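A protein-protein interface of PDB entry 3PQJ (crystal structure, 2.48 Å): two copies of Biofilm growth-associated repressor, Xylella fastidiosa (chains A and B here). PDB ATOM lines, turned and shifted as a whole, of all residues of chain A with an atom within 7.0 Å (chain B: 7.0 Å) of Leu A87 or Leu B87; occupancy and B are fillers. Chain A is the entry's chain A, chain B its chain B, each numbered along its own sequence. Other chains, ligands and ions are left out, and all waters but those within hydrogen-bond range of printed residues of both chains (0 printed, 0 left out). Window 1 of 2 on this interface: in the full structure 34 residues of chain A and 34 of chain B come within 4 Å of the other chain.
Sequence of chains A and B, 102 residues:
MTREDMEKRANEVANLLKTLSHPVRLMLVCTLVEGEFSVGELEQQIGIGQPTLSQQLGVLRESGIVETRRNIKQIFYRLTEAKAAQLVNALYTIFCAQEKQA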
ATOM      1  N   VAL A  13      31.690  14.987  13.845  1.00  0.00           N
ATOM      2  CA  VAL A  13      30.227  15.004  13.750  1.00  0.00           C
ATOM      3  C   VAL A  13      29.683  16.203  14.538  1.00  0.00           C
ATOM      4  O   VAL A  13      28.964  17.018  13.958  1.00  0.00           O
ATOM      5  CB  VAL A  13      29.572  13.667  14.195  1.00  0.00           C
ATOM      6  CG1 VAL A  13      28.053  13.768  14.205  1.00  0.00           C
ATOM      7  CG2 VAL A  13      30.021  12.522  13.296  1.00  0.00           C
ATOM      8  N   LEU A  16      30.269  19.689  12.834  1.00  0.00           N
ATOM      9  CA  LEU A  16      29.347  19.974  11.726  1.00  0.00           C
ATOM     10  C   LEU A  16      27.989  20.396  12.312  1.00  0.00           C
ATOM     11  O   LEU A  16      27.389  21.342  11.829  1.00  0.00           O
ATOM     12  CB  LEU A  16      29.193  18.779  10.752  1.00  0.00           C
ATOM     13  CG  LEU A  16      28.220  18.974   9.539  1.00  0.00           C
ATOM     14  CD1 LEU A  16      28.621  20.153   8.666  1.00  0.00           C
ATOM     15  CD2 LEU A  16      28.126  17.711   8.678  1.00  0.00           C
ATOM     16  N   LEU A  17      27.536  19.725  13.377  1.00  0.00           N
ATOM     17  CA  LEU A  17      26.288  20.059  14.070  1.00  0.00           C
ATOM     18  C   LEU A  17      26.387  21.451  14.705  1.00  0.00           C
ATOM     19  O   LEU A  17      25.436  22.224  14.582  1.00  0.00           O
ATOM     20  CB  LEU A  17      25.869  18.974  15.083  1.00  0.00           C
ATOM     21  CG  LEU A  17      25.668  17.527  14.489  1.00  0.00           C
ATOM     22  CD1 LEU A  17      25.376  16.508  15.562  1.00  0.00           C
ATOM     23  CD2 LEU A  17      24.566  17.463  13.392  1.00  0.00           C
ATOM     24  N   LEU A  20      25.969  24.081  12.056  1.00  0.00           N
ATOM     25  CA  LEU A  20      24.568  24.217  11.647  1.00  0.00           C
ATOM     26  C   LEU A  20      23.577  24.549  12.771  1.00  0.00           C
ATOM     27  O   LEU A  20      22.391  24.717  12.482  1.00  0.00           O
ATOM     28  CB  LEU A  20      24.111  22.970  10.870  1.00  0.00           C
ATOM     29  CG  LEU A  20      25.006  22.510   9.726  1.00  0.00           C
ATOM     30  CD1 LEU A  20      24.588  21.150   9.241  1.00  0.00           C
ATOM     31  CD2 LEU A  20      25.031  23.492   8.584  1.00  0.00           C
ATOM     32  N   ALA A  82      30.312  17.755   1.094  1.00  0.00           N
ATOM     33  CA  ALA A  82      29.246  16.833   0.698  1.00  0.00           C
ATOM     34  C   ALA A  82      28.483  16.290   1.900  1.00  0.00           C
ATOM     35  O   ALA A  82      27.279  16.053   1.785  1.00  0.00           O
ATOM     36  CB  ALA A  82      29.804  15.690  -0.132  1.00  0.00           C
ATOM     37  N   LYS A  83      29.172  16.126   3.052  1.00  0.00           N
ATOM     38  CA  LYS A  83      28.573  15.664   4.317  1.00  0.00           C
ATOM     39  C   LYS A  83      27.495  16.620   4.825  1.00  0.00           C
ATOM     40  O   LYS A  83      26.466  16.157   5.310  1.00  0.00           O
ATOM     41  CB  LYS A  83      29.639  15.414   5.395  1.00  0.00           C
ATOM     42  CG  LYS A  83      30.485  14.178   5.127  1.00  0.00           C
ATOM     43  CD  LYS A  83      31.410  13.895   6.292  1.00  0.00           C
ATOM     44  CE  LYS A  83      32.819  13.523   5.877  1.00  0.00           C
ATOM     45  NZ  LYS A  83      32.883  12.162   5.282  1.00  0.00           N
ATOM     46  N   ALA A  84      27.710  17.942   4.657  1.00  0.00           N
ATOM     47  CA  ALA A  84      26.762  18.985   5.033  1.00  0.00           C
ATOM     48  C   ALA A  84      25.512  18.919   4.136  1.00  0.00           C
ATOM     49  O   ALA A  84      24.393  19.032   4.635  1.00  0.00           O
ATOM     50  CB  ALA A  84      27.421  20.354   4.941  1.00  0.00           C
ATOM     51  N   ALA A  85      25.705  18.693   2.833  1.00  0.00           N
ATOM     52  CA  ALA A  85      24.629  18.571   1.854  1.00  0.00           C
ATOM     53  C   ALA A  85      23.790  17.323   2.163  1.00  0.00           C
ATOM     54  O   ALA A  85      22.561  17.402   2.169  1.00  0.00           O
ATOM     55  CB  ALA A  85      25.214  18.493   0.447  1.00  0.00           C
ATOM     56  N   GLN A  86      24.459  16.181   2.466  1.00  0.00           N
ATOM     57  CA  GLN A  86      23.816  14.913   2.855  1.00  0.00           C
ATOM     58  C   GLN A  86      23.026  15.070   4.167  1.00  0.00           C
ATOM     59  O   GLN A  86      21.938  14.518   4.288  1.00  0.00           O
ATOM     60  CB  GLN A  86      24.849  13.784   2.984  1.00  0.00           C
ATOM     61  CG  GLN A  86      25.361  13.244   1.649  1.00  0.00           C
ATOM     62  CD  GLN A  86      26.627  12.409   1.762  1.00  0.00           C
ATOM     63  OE1 GLN A  86      27.114  12.054   2.847  1.00  0.00           O
ATOM     64  NE2 GLN A  86      27.212  12.091   0.627  1.00  0.00           N
ATOM     65  N   LEU A  87      23.566  15.838   5.131  1.00  0.00           N
ATOM     66  CA  LEU A  87      22.909  16.149   6.409  1.00  0.00           C
ATOM     67  C   LEU A  87      21.663  16.992   6.125  1.00  0.00           C
ATOM     68  O   LEU A  87      20.587  16.656   6.613  1.00  0.00           O
ATOM     69  CB  LEU A  87      23.878  16.848   7.399  1.00  0.00           C
ATOM     70  CG  LEU A  87      23.356  17.303   8.831  1.00  0.00           C
ATOM     71  CD1 LEU A  87      22.542  16.226   9.582  1.00  0.00           C
ATOM     72  CD2 LEU A  87      24.484  17.770   9.705  1.00  0.00           C
ATOM     73  N   VAL A  88      21.786  18.006   5.240  1.00  0.00           N
ATOM     74  CA  VAL A  88      20.658  18.859   4.836  1.00  0.00           C
ATOM     75  C   VAL A  88      19.511  18.042   4.262  1.00  0.00           C
ATOM     76  O   VAL A  88      18.362  18.204   4.683  1.00  0.00           O
ATOM     77  CB  VAL A  88      21.067  20.065   3.954  1.00  0.00           C
ATOM     78  CG1 VAL A  88      19.864  20.636   3.201  1.00  0.00           C
ATOM     79  CG2 VAL A  88      21.703  21.144   4.819  1.00  0.00           C
ATOM     80  N   ASN A  89      19.851  17.096   3.382  1.00  0.00           N
ATOM     81  CA  ASN A  89      18.900  16.191   2.746  1.00  0.00           C
ATOM     82  C   ASN A  89      18.145  15.378   3.796  1.00  0.00           C
ATOM     83  O   ASN A  89      16.919  15.295   3.736  1.00  0.00           O
ATOM     84  CB  ASN A  89      19.624  15.262   1.782  1.00  0.00           C
ATOM     85  CG  ASN A  89      20.111  15.910   0.492  1.00  0.00           C
ATOM     86  OD1 ASN A  89      19.844  17.080   0.158  1.00  0.00           O
ATOM     87  ND2 ASN A  89      20.883  15.154  -0.254  1.00  0.00           N
ATOM     88  N   ALA A  90      18.885  14.787   4.774  1.00  0.00           N
ATOM     89  CA  ALA A  90      18.308  13.981   5.840  1.00  0.00           C
ATOM     90  C   ALA A  90      17.350  14.828   6.680  1.00  0.00           C
ATOM     91  O   ALA A  90      16.282  14.350   7.023  1.00  0.00           O
ATOM     92  CB  ALA A  90      19.409  13.422   6.707  1.00  0.00           C
ATOM     93  N   LEU A  91      17.704  16.106   6.953  1.00  0.00           N
ATOM     94  CA  LEU A  91      16.895  17.043   7.730  1.00  0.00           C
ATOM     95  C   LEU A  91      15.534  17.281   7.093  1.00  0.00           C
ATOM     96  O   LEU A  91      14.555  17.385   7.821  1.00  0.00           O
ATOM     97  CB  LEU A  91      17.654  18.368   8.001  1.00  0.00           C
ATOM     98  CG  LEU A  91      18.872  18.315   8.960  1.00  0.00           C
ATOM     99  CD1 LEU A  91      19.623  19.669   8.971  1.00  0.00           C
ATOM    100  CD2 LEU A  91      18.434  18.071  10.399  1.00  0.00           C
ATOM    101  N   TYR A  92      15.469  17.330   5.739  1.00  0.00           N
ATOM    102  CA  TYR A  92      14.221  17.455   4.958  1.00  0.00           C
ATOM    103  C   TYR A  92      13.318  16.248   5.210  1.00  0.00           C
ATOM    104  O   TYR A  92      12.145  16.415   5.521  1.00  0.00           O
ATOM    105  CB  TYR A  92      14.506  17.617   3.451  1.00  0.00           C
ATOM    106  CG  TYR A  92      14.772  19.061   3.050  1.00  0.00           C
ATOM    107  CD1 TYR A  92      13.737  19.896   2.620  1.00  0.00           C
ATOM    108  CD2 TYR A  92      16.049  19.602   3.134  1.00  0.00           C
ATOM    109  CE1 TYR A  92      13.972  21.239   2.298  1.00  0.00           C
ATOM    110  CE2 TYR A  92      16.297  20.939   2.821  1.00  0.00           C
ATOM    111  CZ  TYR A  92      15.257  21.753   2.398  1.00  0.00           C
ATOM    112  OH  TYR A  92      15.521  23.069   2.097  1.00  0.00           O
ATOM    113  N   ILE A  94      13.412  14.241   7.862  1.00  0.00           N
ATOM    114  CA  ILE A  94      13.021  14.253   9.272  1.00  0.00           C
ATOM    115  C   ILE A  94      12.053  15.395   9.612  1.00  0.00           C
ATOM    116  O   ILE A  94      11.095  15.181  10.348  1.00  0.00           O
ATOM    117  CB  ILE A  94      14.277  14.232  10.203  1.00  0.00           C
ATOM    118  CG1 ILE A  94      15.204  13.027   9.899  1.00  0.00           C
ATOM    119  CG2 ILE A  94      13.915  14.284  11.700  1.00  0.00           C
ATOM    120  CD1 ILE A  94      16.717  13.300  10.227  1.00  0.00           C
ATOM    121  N   PHE A  95      12.301  16.595   9.095  1.00  0.00           N
ATOM    122  CA  PHE A  95      11.523  17.772   9.468  1.00  0.00           C
ATOM    123  C   PHE A  95      10.319  18.153   8.633  1.00  0.00           C
ATOM    124  O   PHE A  95       9.423  18.802   9.159  1.00  0.00           O
ATOM    125  CB  PHE A  95      12.432  18.968   9.819  1.00  0.00           C
ATOM    126  CG  PHE A  95      13.146  18.765  11.135  1.00  0.00           C
ATOM    127  CD1 PHE A  95      12.587  19.225  12.330  1.00  0.00           C
ATOM    128  CD2 PHE A  95      14.346  18.065  11.192  1.00  0.00           C
ATOM    129  CE1 PHE A  95      13.231  19.015  13.550  1.00  0.00           C
ATOM    130  CE2 PHE A  95      14.990  17.854  12.413  1.00  0.00           C
ATOM    131  CZ  PHE A  95      14.421  18.324  13.584  1.00  0.00           C
ATOM    132  N   VAL B  13      14.923  23.039  14.219  1.00  0.00           N
ATOM    133  CA  VAL B  13      15.984  22.221  13.620  1.00  0.00           C
ATOM    134  C   VAL B  13      17.315  22.605  14.261  1.00  0.00           C
ATOM    135  O   VAL B  13      17.991  21.727  14.789  1.00  0.00           O
ATOM    136  CB  VAL B  13      16.035  22.317  12.061  1.00  0.00           C
ATOM    137  CG1 VAL B  13      17.211  21.535  11.496  1.00  0.00           C
ATOM    138  CG2 VAL B  13      14.739  21.839  11.432  1.00  0.00           C
ATOM    139  N   LEU B  16      17.794  21.322  17.941  1.00  0.00           N
ATOM    140  CA  LEU B  16      18.120  19.892  18.045  1.00  0.00           C
ATOM    141  C   LEU B  16      19.598  19.698  17.699  1.00  0.00           C
ATOM    142  O   LEU B  16      20.288  18.948  18.394  1.00  0.00           O
ATOM    143  CB  LEU B  16      17.220  18.999  17.150  1.00  0.00           C
ATOM    144  CG  LEU B  16      17.512  17.467  17.159  1.00  0.00           C
ATOM    145  CD1 LEU B  16      17.377  16.870  18.535  1.00  0.00           C
ATOM    146  CD2 LEU B  16      16.632  16.721  16.180  1.00  0.00           C
ATOM    147  N   LEU B  17      20.093  20.413  16.663  1.00  0.00           N
ATOM    148  CA  LEU B  17      21.497  20.351  16.264  1.00  0.00           C
ATOM    149  C   LEU B  17      22.379  20.906  17.396  1.00  0.00           C
ATOM    150  O   LEU B  17      23.421  20.328  17.674  1.00  0.00           O
ATOM    151  CB  LEU B  17      21.748  21.054  14.913  1.00  0.00           C
ATOM    152  CG  LEU B  17      20.944  20.525  13.703  1.00  0.00           C
ATOM    153  CD1 LEU B  17      21.190  21.354  12.463  1.00  0.00           C
ATOM    154  CD2 LEU B  17      21.299  19.121  13.374  1.00  0.00           C
ATOM    155  N   LEU B  20      22.752  18.254  20.094  1.00  0.00           N
ATOM    156  CA  LEU B  20      23.706  17.223  19.680  1.00  0.00           C
ATOM    157  C   LEU B  20      25.120  17.748  19.306  1.00  0.00           C
ATOM    158  O   LEU B  20      25.991  16.950  18.953  1.00  0.00           O
ATOM    159  CB  LEU B  20      23.122  16.399  18.527  1.00  0.00           C
ATOM    160  CG  LEU B  20      21.715  15.846  18.695  1.00  0.00           C
ATOM    161  CD1 LEU B  20      21.195  15.339  17.377  1.00  0.00           C
ATOM    162  CD2 LEU B  20      21.665  14.763  19.761  1.00  0.00           C
ATOM    163  N   LEU B  26      26.078  13.834  22.005  1.00  0.00           N
ATOM    164  CA  LEU B  26      25.934  13.049  20.780  1.00  0.00           C
ATOM    165  C   LEU B  26      26.099  11.548  21.052  1.00  0.00           C
ATOM    166  O   LEU B  26      25.257  10.762  20.608  1.00  0.00           O
ATOM    167  CB  LEU B  26      26.959  13.535  19.735  1.00  0.00           C
ATOM    168  CG  LEU B  26      27.060  12.743  18.435  1.00  0.00           C
ATOM    169  CD1 LEU B  26      25.806  12.921  17.561  1.00  0.00           C
ATOM    170  CD2 LEU B  26      28.300  13.113  17.710  1.00  0.00           C
ATOM    171  N   ALA B  82      11.814  11.065  18.575  1.00  0.00           N
ATOM    172  CA  ALA B  82      12.087  10.215  17.412  1.00  0.00           C
ATOM    173  C   ALA B  82      12.928  10.928  16.369  1.00  0.00           C
ATOM    174  O   ALA B  82      13.720  10.266  15.700  1.00  0.00           O
ATOM    175  CB  ALA B  82      10.799   9.704  16.802  1.00  0.00           C
ATOM    176  N   LYS B  83      12.800  12.275  16.269  1.00  0.00           N
ATOM    177  CA  LYS B  83      13.582  13.121  15.359  1.00  0.00           C
ATOM    178  C   LYS B  83      15.083  13.039  15.661  1.00  0.00           C
ATOM    179  O   LYS B  83      15.890  13.014  14.732  1.00  0.00           O
ATOM    180  CB  LYS B  83      13.095  14.580  15.377  1.00  0.00           C
ATOM    181  CG  LYS B  83      11.766  14.779  14.672  1.00  0.00           C
ATOM    182  CD  LYS B  83      11.414  16.247  14.586  1.00  0.00           C
ATOM    183  CE  LYS B  83       9.980  16.571  14.951  1.00  0.00           C
ATOM    184  NZ  LYS B  83       9.035  16.161  13.883  1.00  0.00           N
ATOM    185  N   ALA B  84      15.449  12.946  16.954  1.00  0.00           N
ATOM    186  CA  ALA B  84      16.837  12.803  17.411  1.00  0.00           C
ATOM    187  C   ALA B  84      17.391  11.443  16.987  1.00  0.00           C
ATOM    188  O   ALA B  84      18.511  11.367  16.494  1.00  0.00           O
ATOM    189  CB  ALA B  84      16.909  12.959  18.928  1.00  0.00           C
ATOM    190  N   ALA B  85      16.580  10.385  17.111  1.00  0.00           N
ATOM    191  CA  ALA B  85      16.946   9.028  16.721  1.00  0.00           C
ATOM    192  C   ALA B  85      17.177   8.954  15.218  1.00  0.00           C
ATOM    193  O   ALA B  85      18.190   8.399  14.791  1.00  0.00           O
ATOM    194  CB  ALA B  85      15.859   8.045  17.151  1.00  0.00           C
ATOM    195  N   GLN B  86      16.258   9.533  14.422  1.00  0.00           N
ATOM    196  CA  GLN B  86      16.379   9.584  12.951  1.00  0.00           C
ATOM    197  C   GLN B  86      17.597  10.400  12.505  1.00  0.00           C
ATOM    198  O   GLN B  86      18.269  10.004  11.548  1.00  0.00           O
ATOM    199  CB  GLN B  86      15.094  10.124  12.304  1.00  0.00           C
ATOM    200  CG  GLN B  86      13.848   9.281  12.632  1.00  0.00           C
ATOM    201  CD  GLN B  86      12.562  10.016  12.377  1.00  0.00           C
ATOM    202  OE1 GLN B  86      12.508  11.245  12.339  1.00  0.00           O
ATOM    203  NE2 GLN B  86      11.497   9.281  12.201  1.00  0.00           N
ATOM    204  N   LEU B  87      17.909  11.503  13.227  1.00  0.00           N
ATOM    205  CA  LEU B  87      19.089  12.344  12.960  1.00  0.00           C
ATOM    206  C   LEU B  87      20.359  11.541  13.250  1.00  0.00           C
ATOM    207  O   LEU B  87      21.255  11.471  12.399  1.00  0.00           O
ATOM    208  CB  LEU B  87      19.030  13.618  13.821  1.00  0.00           C
ATOM    209  CG  LEU B  87      19.794  14.861  13.391  1.00  0.00           C
ATOM    210  CD1 LEU B  87      21.190  14.846  13.861  1.00  0.00           C
ATOM    211  CD2 LEU B  87      19.720  15.110  11.896  1.00  0.00           C
ATOM    212  N   VAL B  88      20.403  10.910  14.438  1.00  0.00           N
ATOM    213  CA  VAL B  88      21.489  10.044  14.893  1.00  0.00           C
ATOM    214  C   VAL B  88      21.750   8.926  13.864  1.00  0.00           C
ATOM    215  O   VAL B  88      22.900   8.731  13.477  1.00  0.00           O
ATOM    216  CB  VAL B  88      21.284   9.598  16.376  1.00  0.00           C
ATOM    217  CG1 VAL B  88      21.899   8.245  16.672  1.00  0.00           C
ATOM    218  CG2 VAL B  88      21.847  10.654  17.320  1.00  0.00           C
ATOM    219  N   ASN B  89      20.663   8.307  13.333  1.00  0.00           N
ATOM    220  CA  ASN B  89      20.697   7.277  12.287  1.00  0.00           C
ATOM    221  C   ASN B  89      21.321   7.744  10.987  1.00  0.00           C
ATOM    222  O   ASN B  89      22.095   6.992  10.387  1.00  0.00           O
ATOM    223  CB  ASN B  89      19.288   6.757  12.004  1.00  0.00           C
ATOM    224  CG  ASN B  89      18.754   5.813  13.049  1.00  0.00           C
ATOM    225  OD1 ASN B  89      19.376   5.557  14.083  1.00  0.00           O
ATOM    226  ND2 ASN B  89      17.553   5.326  12.816  1.00  0.00           N
ATOM    227  N   ALA B  90      20.936   8.956  10.518  1.00  0.00           N
ATOM    228  CA  ALA B  90      21.420   9.596   9.297  1.00  0.00           C
ATOM    229  C   ALA B  90      22.903   9.896   9.407  1.00  0.00           C
ATOM    230  O   ALA B  90      23.636   9.688   8.443  1.00  0.00           O
ATOM    231  CB  ALA B  90      20.645  10.875   9.038  1.00  0.00           C
ATOM    232  N   LEU B  91      23.356  10.328  10.591  1.00  0.00           N
ATOM    233  CA  LEU B  91      24.764  10.624  10.874  1.00  0.00           C
ATOM    234  C   LEU B  91      25.675   9.421  10.667  1.00  0.00           C
ATOM    235  O   LEU B  91      26.784   9.594  10.154  1.00  0.00           O
ATOM    236  CB  LEU B  91      24.950  11.234  12.278  1.00  0.00           C
ATOM    237  CG  LEU B  91      24.346  12.635  12.511  1.00  0.00           C
ATOM    238  CD1 LEU B  91      24.509  13.067  13.960  1.00  0.00           C
ATOM    239  CD2 LEU B  91      24.833  13.667  11.487  1.00  0.00           C
ATOM    240  N   TYR B  92      25.196   8.202  11.010  1.00  0.00           N
ATOM    241  CA  TYR B  92      25.916   6.939  10.788  1.00  0.00           C
ATOM    242  C   TYR B  92      26.120   6.714   9.292  1.00  0.00           C
ATOM    243  O   TYR B  92      27.232   6.422   8.871  1.00  0.00           O
ATOM    244  CB  TYR B  92      25.148   5.749  11.379  1.00  0.00           C
ATOM    245  CG  TYR B  92      25.425   5.488  12.832  1.00  0.00           C
ATOM    246  CD1 TYR B  92      26.380   4.555  13.222  1.00  0.00           C
ATOM    247  CD2 TYR B  92      24.726   6.163  13.824  1.00  0.00           C
ATOM    248  CE1 TYR B  92      26.625   4.287  14.568  1.00  0.00           C
ATOM    249  CE2 TYR B  92      24.963   5.909  15.172  1.00  0.00           C
ATOM    250  CZ  TYR B  92      25.910   4.967  15.540  1.00  0.00           C
ATOM    251  OH  TYR B  92      26.148   4.743  16.872  1.00  0.00           O
ATOM    252  N   ILE B  94      26.127   9.019   6.901  1.00  0.00           N
ATOM    253  CA  ILE B  94      27.010  10.075   6.397  1.00  0.00           C
ATOM    254  C   ILE B  94      28.456   9.939   6.905  1.00  0.00           C
ATOM    255  O   ILE B  94      29.396  10.120   6.136  1.00  0.00           O
ATOM    256  CB  ILE B  94      26.405  11.494   6.674  1.00  0.00           C
ATOM    257  CG1 ILE B  94      24.979  11.638   6.094  1.00  0.00           C
ATOM    258  CG2 ILE B  94      27.312  12.620   6.178  1.00  0.00           C
ATOM    259  CD1 ILE B  94      24.086  12.632   6.881  1.00  0.00           C
ATOM    260  N   PHE B  95      28.635   9.648   8.185  1.00  0.00           N
ATOM    261  CA  PHE B  95      29.969   9.639   8.778  1.00  0.00           C
ATOM    262  C   PHE B  95      30.752   8.347   8.818  1.00  0.00           C
ATOM    263  O   PHE B  95      31.981   8.413   8.881  1.00  0.00           O
ATOM    264  CB  PHE B  95      29.988  10.400  10.112  1.00  0.00           C
ATOM    265  CG  PHE B  95      29.855  11.888   9.914  1.00  0.00           C
ATOM    266  CD1 PHE B  95      30.982  12.696   9.834  1.00  0.00           C
ATOM    267  CD2 PHE B  95      28.606  12.480   9.789  1.00  0.00           C
ATOM    268  CE1 PHE B  95      30.857  14.072   9.666  1.00  0.00           C
ATOM    269  CE2 PHE B  95      28.485  13.856   9.591  1.00  0.00           C
ATOM    270  CZ  PHE B  95      29.612  14.640   9.539  1.00  0.00           C
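Hydrophobic or aromatic side chains of chain A that line the printed part of chain B: Val A13, Leu A16, Leu A17, Leu A20, Leu A87, Ala A90, Leu A91, Ile A94 and Phe A95.
Lys A83 touches Ile B94, and with the chains exchanged Ile A94 touches Lys B83.
Lys A83 touches Phe B95, and with the chains exchanged Phe A95 touches Lys B83.
Leu A87 touches Ile B94, and with the chains exchanged Ile A94 touches Leu B87.
Ala A90 touches its own counterpart, Ala B90.
Of the 23 pairs that touch across the chains among the printed residues, 21 have their exchanged pair printed and touching as well.
Val A13 touches Leu B91.
Val A13 touches Phe B95.
Leu A17 touches Leu B17.
Leu B91 touches Leu A17.
Lys A83 touches Ile B94 (CG to CG2, 3.7 Å).
CD2 of Leu B87 touches CD1 of Leu A87, 3.8 Å away.
Ile B94 touches Leu A87 (CD1 to N, 3.7 Å).
Leu A91 touches Leu B87 (CD2 to CD2, 3.6 Å).
Leu B87 touches Ile A94.
Phe A95 touches Lys B83 (CE1 to CD, 3.5 Å).
Leu A87 touches just these residues of chain B: Leu B87 (3.8 Å), Leu B91 (3.9 Å) and Ile B94 (3.7 Å).
Of the printed residues of chain A, Leu B16 touches Phe A95 (3.8 Å).
Printed residues of chain A within 4 Å of Leu B20: Leu A17 (3.5 Å).
Ala B82 touches none of the printed residues of chain A.
Printed residues of chain A within 4 Å of Leu B87: Leu A87, Leu A91 and Ile A94.
Val B88 touches none of the printed residues of chain A.
Of the printed residues of chain A, Leu B91 touches Val A13 (3.6 Å), Leu A17 (3.9 Å) and Leu A87 (3.9 Å).
Of the printed residues of chain A, Ile B94 touches Lys A83 (3.7 Å), Gln A86 (3.4 Å) and Leu A87 (3.7 Å).
The nearest residue of chain B that does not touch Leu A87 is Leu B17 (4.9 Å).
The nearest residue of chain A that does not touch Leu B87 is Leu A17 (4.3 Å).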
